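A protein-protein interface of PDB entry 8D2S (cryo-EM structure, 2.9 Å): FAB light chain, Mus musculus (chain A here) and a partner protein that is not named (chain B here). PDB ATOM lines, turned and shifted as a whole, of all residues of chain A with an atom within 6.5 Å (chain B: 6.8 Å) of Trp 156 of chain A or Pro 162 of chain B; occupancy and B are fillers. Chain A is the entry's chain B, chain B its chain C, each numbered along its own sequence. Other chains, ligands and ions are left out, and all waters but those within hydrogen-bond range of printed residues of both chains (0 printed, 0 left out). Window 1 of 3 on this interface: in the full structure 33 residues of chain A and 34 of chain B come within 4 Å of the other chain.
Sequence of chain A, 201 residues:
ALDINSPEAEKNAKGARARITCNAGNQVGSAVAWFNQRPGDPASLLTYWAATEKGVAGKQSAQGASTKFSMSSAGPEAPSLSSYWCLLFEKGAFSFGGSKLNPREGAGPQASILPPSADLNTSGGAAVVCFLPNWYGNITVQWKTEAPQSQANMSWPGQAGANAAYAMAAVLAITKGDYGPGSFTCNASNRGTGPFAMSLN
The backbone NH (N) of Met 154 of chain A lies within hydrogen-bond range of the side-chain carboxylate (OE1) of Glu 164 of chain B (3.3 Å).
N of Ser 155 of chain A is in hydrogen-bond range of O of Ala 169 of chain A (2.9 Å). NE1 of Trp 156 of chain A sits at hydrogen-bond distance from SD of Met 168 of chain A (3.1 Å). N of Phe 161 of chain B sits at hydrogen-bond distance from O of Ala 173 of chain B. O of Glu 164 of chain B lies within hydrogen-bond range of N of Asn 171 of chain B, 2.9 Å away.
CB of Phe 161 of chain B touches OG of Ser 155 of chain A, at 3.4 Å. Pro 162 of chain B touches Ser 155 of chain A. Pro 162 of chain B touches Trp 156 of chain A (CG to O, 3.3 Å). CG of Pro 157 of chain A touches CD1 of Phe 161 of chain B, 3.5 Å away. Pro 162 of chain B touches Pro 157 of chain A. Phe 161 of chain B touches Ala 167 of chain A. Met 168 of chain A touches Phe 161 of chain B (C to CE1, 3.4 Å). CB of Ala 169 of chain A touches CG of Phe 161 of chain B (3.5 Å).
Trp 156 of chain A touches one residue of chain B. Of chain A, only Ser 155 (3.4 Å), Trp 156 (3.3 Å) and Pro 157 (3.7 Å) come within 4 Å of Pro 162 of chain B. Printed residues of chain B within 4 Å of Ser 155 of chain A: Phe 161 and Pro 162. Printed residues of chain B within 4 Å of Pro 157 of chain A: Phe 161 and Pro 162. Printed residues of chain B within 4 Å of Ala 169 of chain A: Phe 161 (3.5 Å). Printed residues of chain B within 4 Å of Ala 167 of chain A: Phe 161. Printed residues of chain B within 4 Å of Met 154 of chain A: Glu 164. The nearest residue of chain A that does not touch Pro 162 of chain B is Gly 158 of chain A (5.6 Å). The nearest printed residue of chain B that does not touch Met 168 of chain A is Ala 173 of chain B (7.5 Å).
Hydrophobic or aromatic side chains of chain A that line the printed part of chain B: Pro 157, Ala 167 and Ala 169. Of the 10 printed residues of chain B, 3 touch a printed residue of chain A. Hydrophobic or aromatic side chains of chain B within 4 Å of the printed part of chain A: Phe 161 and Pro 162. Among the printed residues, no Asp or Glu carboxylate lies within 4 Å of a Lys or Arg side-chain nitrogen of the other chain.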
ATOM      1  N   TRP A 135      23.509   3.391 -40.482  1.00  0.00           N
ATOM      2  CA  TRP A 135      24.476   2.887 -41.447  1.00  0.00           C
ATOM      3  C   TRP A 135      23.888   1.645 -42.098  1.00  0.00           C
ATOM      4  O   TRP A 135      22.917   1.065 -41.608  1.00  0.00           O
ATOM      5  CB  TRP A 135      25.830   2.588 -40.793  1.00  0.00           C
ATOM      6  CG  TRP A 135      25.731   1.968 -39.437  1.00  0.00           C
ATOM      7  CD1 TRP A 135      25.658   2.621 -38.243  1.00  0.00           C
ATOM      8  CD2 TRP A 135      25.709   0.570 -39.131  1.00  0.00           C
ATOM      9  NE1 TRP A 135      25.584   1.718 -37.213  1.00  0.00           N
ATOM     10  CE2 TRP A 135      25.615   0.451 -37.732  1.00  0.00           C
ATOM     11  CE3 TRP A 135      25.757  -0.592 -39.904  1.00  0.00           C
ATOM     12  CZ2 TRP A 135      25.566  -0.783 -37.091  1.00  0.00           C
ATOM     13  CZ3 TRP A 135      25.709  -1.816 -39.265  1.00  0.00           C
ATOM     14  CH2 TRP A 135      25.615  -1.902 -37.873  1.00  0.00           C
ATOM     15  N   ILE A 139      29.654  -3.187 -39.215  1.00  0.00           N
ATOM     16  CA  ILE A 139      30.540  -2.194 -38.626  1.00  0.00           C
ATOM     17  C   ILE A 139      31.178  -2.773 -37.369  1.00  0.00           C
ATOM     18  O   ILE A 139      30.681  -3.733 -36.775  1.00  0.00           O
ATOM     19  CB  ILE A 139      29.790  -0.873 -38.317  1.00  0.00           C
ATOM     20  CG1 ILE A 139      30.725   0.328 -38.453  1.00  0.00           C
ATOM     21  CG2 ILE A 139      29.162  -0.903 -36.935  1.00  0.00           C
ATOM     22  CD1 ILE A 139      30.006   1.651 -38.394  1.00  0.00           C
ATOM     23  N   MET A 154      28.063  -4.852 -26.674  1.00  0.00           N
ATOM     24  CA  MET A 154      27.545  -4.275 -27.905  1.00  0.00           C
ATOM     25  C   MET A 154      26.185  -4.871 -28.241  1.00  0.00           C
ATOM     26  O   MET A 154      25.956  -6.069 -28.050  1.00  0.00           O
ATOM     27  CB  MET A 154      28.523  -4.511 -29.059  1.00  0.00           C
ATOM     28  CG  MET A 154      29.925  -3.983 -28.787  1.00  0.00           C
ATOM     29  SD  MET A 154      31.172  -4.670 -29.891  1.00  0.00           S
ATOM     30  CE  MET A 154      32.642  -3.834 -29.301  1.00  0.00           C
ATOM     31  N   SER A 155      25.287  -4.026 -28.741  1.00  0.00           N
ATOM     32  CA  SER A 155      23.951  -4.448 -29.136  1.00  0.00           C
ATOM     33  C   SER A 155      23.612  -3.847 -30.493  1.00  0.00           C
ATOM     34  O   SER A 155      24.041  -2.739 -30.823  1.00  0.00           O
ATOM     35  CB  SER A 155      22.896  -4.042 -28.099  1.00  0.00           C
ATOM     36  OG  SER A 155      22.889  -2.640 -27.900  1.00  0.00           O
ATOM     37  N   TRP A 156      22.831  -4.594 -31.275  1.00  0.00           N
ATOM     38  CA  TRP A 156      22.451  -4.194 -32.621  1.00  0.00           C
ATOM     39  C   TRP A 156      20.950  -4.391 -32.803  1.00  0.00           C
ATOM     40  O   TRP A 156      20.435  -5.491 -32.538  1.00  0.00           O
ATOM     41  CB  TRP A 156      23.205  -5.008 -33.680  1.00  0.00           C
ATOM     42  CG  TRP A 156      24.688  -5.009 -33.531  1.00  0.00           C
ATOM     43  CD1 TRP A 156      25.574  -4.195 -34.170  1.00  0.00           C
ATOM     44  CD2 TRP A 156      25.467  -5.879 -32.703  1.00  0.00           C
ATOM     45  NE1 TRP A 156      26.856  -4.498 -33.787  1.00  0.00           N
ATOM     46  CE2 TRP A 156      26.817  -5.528 -32.884  1.00  0.00           C
ATOM     47  CE3 TRP A 156      25.152  -6.917 -31.821  1.00  0.00           C
ATOM     48  CZ2 TRP A 156      27.853  -6.178 -32.218  1.00  0.00           C
ATOM     49  CZ3 TRP A 156      26.180  -7.560 -31.160  1.00  0.00           C
ATOM     50  CH2 TRP A 156      27.514  -7.189 -31.362  1.00  0.00           C
ATOM     51  N   PRO A 157      20.221  -3.379 -33.255  1.00  0.00           N
ATOM     52  CA  PRO A 157      18.830  -3.579 -33.666  1.00  0.00           C
ATOM     53  C   PRO A 157      18.777  -4.269 -35.026  1.00  0.00           C
ATOM     54  O   PRO A 157      19.795  -4.611 -35.623  1.00  0.00           O
ATOM     55  CB  PRO A 157      18.267  -2.154 -33.746  1.00  0.00           C
ATOM     56  CG  PRO A 157      19.262  -1.286 -33.058  1.00  0.00           C
ATOM     57  CD  PRO A 157      20.583  -1.955 -33.236  1.00  0.00           C
ATOM     58  N   GLY A 158      17.556  -4.459 -35.516  1.00  0.00           N
ATOM     59  CA  GLY A 158      17.370  -4.996 -36.848  1.00  0.00           C
ATOM     60  C   GLY A 158      17.553  -3.935 -37.911  1.00  0.00           C
ATOM     61  O   GLY A 158      18.422  -3.066 -37.789  1.00  0.00           O
ATOM     62  N   ALA A 167      21.675   0.162 -36.733  1.00  0.00           N
ATOM     63  CA  ALA A 167      22.218   0.934 -35.627  1.00  0.00           C
ATOM     64  C   ALA A 167      23.088   0.031 -34.763  1.00  0.00           C
ATOM     65  O   ALA A 167      23.175  -1.180 -34.981  1.00  0.00           O
ATOM     66  CB  ALA A 167      21.104   1.569 -34.785  1.00  0.00           C
ATOM     67  N   MET A 168      23.739   0.636 -33.770  1.00  0.00           N
ATOM     68  CA  MET A 168      24.599  -0.106 -32.859  1.00  0.00           C
ATOM     69  C   MET A 168      24.818   0.716 -31.599  1.00  0.00           C
ATOM     70  O   MET A 168      24.964   1.938 -31.666  1.00  0.00           O
ATOM     71  CB  MET A 168      25.944  -0.442 -33.515  1.00  0.00           C
ATOM     72  CG  MET A 168      26.857  -1.297 -32.656  1.00  0.00           C
ATOM     73  SD  MET A 168      28.358  -1.795 -33.512  1.00  0.00           S
ATOM     74  CE  MET A 168      29.192  -2.702 -32.216  1.00  0.00           C
ATOM     75  N   ALA A 169      24.833   0.042 -30.453  1.00  0.00           N
ATOM     76  CA  ALA A 169      25.153   0.674 -29.180  1.00  0.00           C
ATOM     77  C   ALA A 169      26.293  -0.095 -28.532  1.00  0.00           C
ATOM     78  O   ALA A 169      26.181  -1.305 -28.313  1.00  0.00           O
ATOM     79  CB  ALA A 169      23.937   0.713 -28.256  1.00  0.00           C
ATOM     80  N   TYR B 144      18.093  -4.691 -14.635  1.00  0.00           N
ATOM     81  CA  TYR B 144      16.752  -5.231 -14.467  1.00  0.00           C
ATOM     82  C   TYR B 144      16.731  -6.673 -14.957  1.00  0.00           C
ATOM     83  O   TYR B 144      17.672  -7.143 -15.600  1.00  0.00           O
ATOM     84  CB  TYR B 144      15.711  -4.380 -15.206  1.00  0.00           C
ATOM     85  CG  TYR B 144      15.949  -4.244 -16.693  1.00  0.00           C
ATOM     86  CD1 TYR B 144      16.750  -3.228 -17.198  1.00  0.00           C
ATOM     87  CD2 TYR B 144      15.362  -5.122 -17.591  1.00  0.00           C
ATOM     88  CE1 TYR B 144      16.967  -3.102 -18.556  1.00  0.00           C
ATOM     89  CE2 TYR B 144      15.575  -5.002 -18.946  1.00  0.00           C
ATOM     90  CZ  TYR B 144      16.376  -3.991 -19.424  1.00  0.00           C
ATOM     91  OH  TYR B 144      16.582  -3.875 -20.777  1.00  0.00           O
ATOM     92  N   THR B 160      15.603   2.051 -29.970  1.00  0.00           N
ATOM     93  CA  THR B 160      15.741   1.293 -28.731  1.00  0.00           C
ATOM     94  C   THR B 160      16.529   0.025 -29.030  1.00  0.00           C
ATOM     95  O   THR B 160      16.029  -0.885 -29.699  1.00  0.00           O
ATOM     96  CB  THR B 160      14.375   0.967 -28.133  1.00  0.00           C
ATOM     97  OG1 THR B 160      13.605   0.217 -29.081  1.00  0.00           O
ATOM     98  CG2 THR B 160      13.631   2.246 -27.779  1.00  0.00           C
ATOM     99  N   PHE B 161      17.762  -0.029 -28.538  1.00  0.00           N
ATOM    100  CA  PHE B 161      18.632  -1.157 -28.811  1.00  0.00           C
ATOM    101  C   PHE B 161      18.206  -2.367 -27.980  1.00  0.00           C
ATOM    102  O   PHE B 161      17.661  -2.213 -26.884  1.00  0.00           O
ATOM    103  CB  PHE B 161      20.081  -0.784 -28.512  1.00  0.00           C
ATOM    104  CG  PHE B 161      20.553   0.431 -29.257  1.00  0.00           C
ATOM    105  CD1 PHE B 161      21.094   0.314 -30.523  1.00  0.00           C
ATOM    106  CD2 PHE B 161      20.445   1.693 -28.697  1.00  0.00           C
ATOM    107  CE1 PHE B 161      21.520   1.429 -31.217  1.00  0.00           C
ATOM    108  CE2 PHE B 161      20.868   2.811 -29.386  1.00  0.00           C
ATOM    109  CZ  PHE B 161      21.409   2.679 -30.647  1.00  0.00           C
ATOM    110  N   PRO B 162      18.417  -3.579 -28.493  1.00  0.00           N
ATOM    111  CA  PRO B 162      18.041  -4.776 -27.733  1.00  0.00           C
ATOM    112  C   PRO B 162      18.840  -4.913 -26.447  1.00  0.00           C
ATOM    113  O   PRO B 162      20.007  -4.524 -26.363  1.00  0.00           O
ATOM    114  CB  PRO B 162      18.351  -5.923 -28.703  1.00  0.00           C
ATOM    115  CG  PRO B 162      18.304  -5.297 -30.051  1.00  0.00           C
ATOM    116  CD  PRO B 162      18.839  -3.911 -29.864  1.00  0.00           C
ATOM    117  N   SER B 163      18.185  -5.475 -25.436  1.00  0.00           N
ATOM    118  CA  SER B 163      18.808  -5.644 -24.133  1.00  0.00           C
ATOM    119  C   SER B 163      19.857  -6.750 -24.170  1.00  0.00           C
ATOM    120  O   SER B 163      19.773  -7.695 -24.959  1.00  0.00           O
ATOM    121  CB  SER B 163      17.748  -5.953 -23.078  1.00  0.00           C
ATOM    122  OG  SER B 163      16.896  -7.001 -23.507  1.00  0.00           O
ATOM    123  N   GLU B 164      20.855  -6.621 -23.299  1.00  0.00           N
ATOM    124  CA  GLU B 164      21.976  -7.548 -23.253  1.00  0.00           C
ATOM    125  C   GLU B 164      22.260  -7.918 -21.804  1.00  0.00           C
ATOM    126  O   GLU B 164      21.938  -7.173 -20.880  1.00  0.00           O
ATOM    127  CB  GLU B 164      23.225  -6.936 -23.897  1.00  0.00           C
ATOM    128  CG  GLU B 164      23.634  -5.617 -23.268  1.00  0.00           C
ATOM    129  CD  GLU B 164      24.765  -4.942 -24.008  1.00  0.00           C
ATOM    130  OE1 GLU B 164      25.255  -5.520 -25.001  1.00  0.00           O
ATOM    131  OE2 GLU B 164      25.168  -3.834 -23.595  1.00  0.00           O
ATOM    132  N   TRP B 170      20.092  -7.091 -17.107  1.00  0.00           N
ATOM    133  CA  TRP B 170      19.944  -6.643 -18.482  1.00  0.00           C
ATOM    134  C   TRP B 170      20.253  -5.154 -18.604  1.00  0.00           C
ATOM    135  O   TRP B 170      19.976  -4.359 -17.698  1.00  0.00           O
ATOM    136  CB  TRP B 170      18.531  -6.921 -19.006  1.00  0.00           C
ATOM    137  CG  TRP B 170      18.122  -8.369 -18.989  1.00  0.00           C
ATOM    138  CD1 TRP B 170      17.762  -9.106 -17.899  1.00  0.00           C
ATOM    139  CD2 TRP B 170      18.004  -9.245 -20.118  1.00  0.00           C
ATOM    140  NE1 TRP B 170      17.441 -10.387 -18.275  1.00  0.00           N
ATOM    141  CE2 TRP B 170      17.579 -10.498 -19.632  1.00  0.00           C
ATOM    142  CE3 TRP B 170      18.222  -9.093 -21.489  1.00  0.00           C
ATOM    143  CZ2 TRP B 170      17.370 -11.590 -20.470  1.00  0.00           C
ATOM    144  CZ3 TRP B 170      18.011 -10.178 -22.320  1.00  0.00           C
ATOM    145  CH2 TRP B 170      17.589 -11.411 -21.807  1.00  0.00           C
ATOM    146  N   ASN B 171      20.835  -4.793 -19.743  1.00  0.00           N
ATOM    147  CA  ASN B 171      21.177  -3.422 -20.082  1.00  0.00           C
ATOM    148  C   ASN B 171      20.561  -3.066 -21.428  1.00  0.00           C
ATOM    149  O   ASN B 171      20.438  -3.913 -22.318  1.00  0.00           O
ATOM    150  CB  ASN B 171      22.697  -3.224 -20.128  1.00  0.00           C
ATOM    151  CG  ASN B 171      23.094  -1.770 -20.302  1.00  0.00           C
ATOM    152  OD1 ASN B 171      23.223  -1.030 -19.328  1.00  0.00           O
ATOM    153  ND2 ASN B 171      23.295  -1.355 -21.547  1.00  0.00           N
ATOM    154  N   LEU B 172      20.175  -1.800 -21.566  1.00  0.00           N
ATOM    155  CA  LEU B 172      19.482  -1.320 -22.749  1.00  0.00           C
ATOM    156  C   LEU B 172      19.796   0.158 -22.923  1.00  0.00           C
ATOM    157  O   LEU B 172      20.084   0.864 -21.953  1.00  0.00           O
ATOM    158  CB  LEU B 172      17.970  -1.556 -22.627  1.00  0.00           C
ATOM    159  CG  LEU B 172      17.034  -1.268 -23.801  1.00  0.00           C
ATOM    160  CD1 LEU B 172      15.981  -2.355 -23.912  1.00  0.00           C
ATOM    161  CD2 LEU B 172      16.373   0.088 -23.638  1.00  0.00           C
ATOM    162  N   ALA B 173      19.742   0.624 -24.168  1.00  0.00           N
ATOM    163  CA  ALA B 173      20.023   2.017 -24.474  1.00  0.00           C
ATOM    164  C   ALA B 173      18.992   2.540 -25.462  1.00  0.00           C
ATOM    165  O   ALA B 173      18.422   1.783 -26.251  1.00  0.00           O
ATOM    166  CB  ALA B 173      21.436   2.195 -25.041  1.00  0.00           C
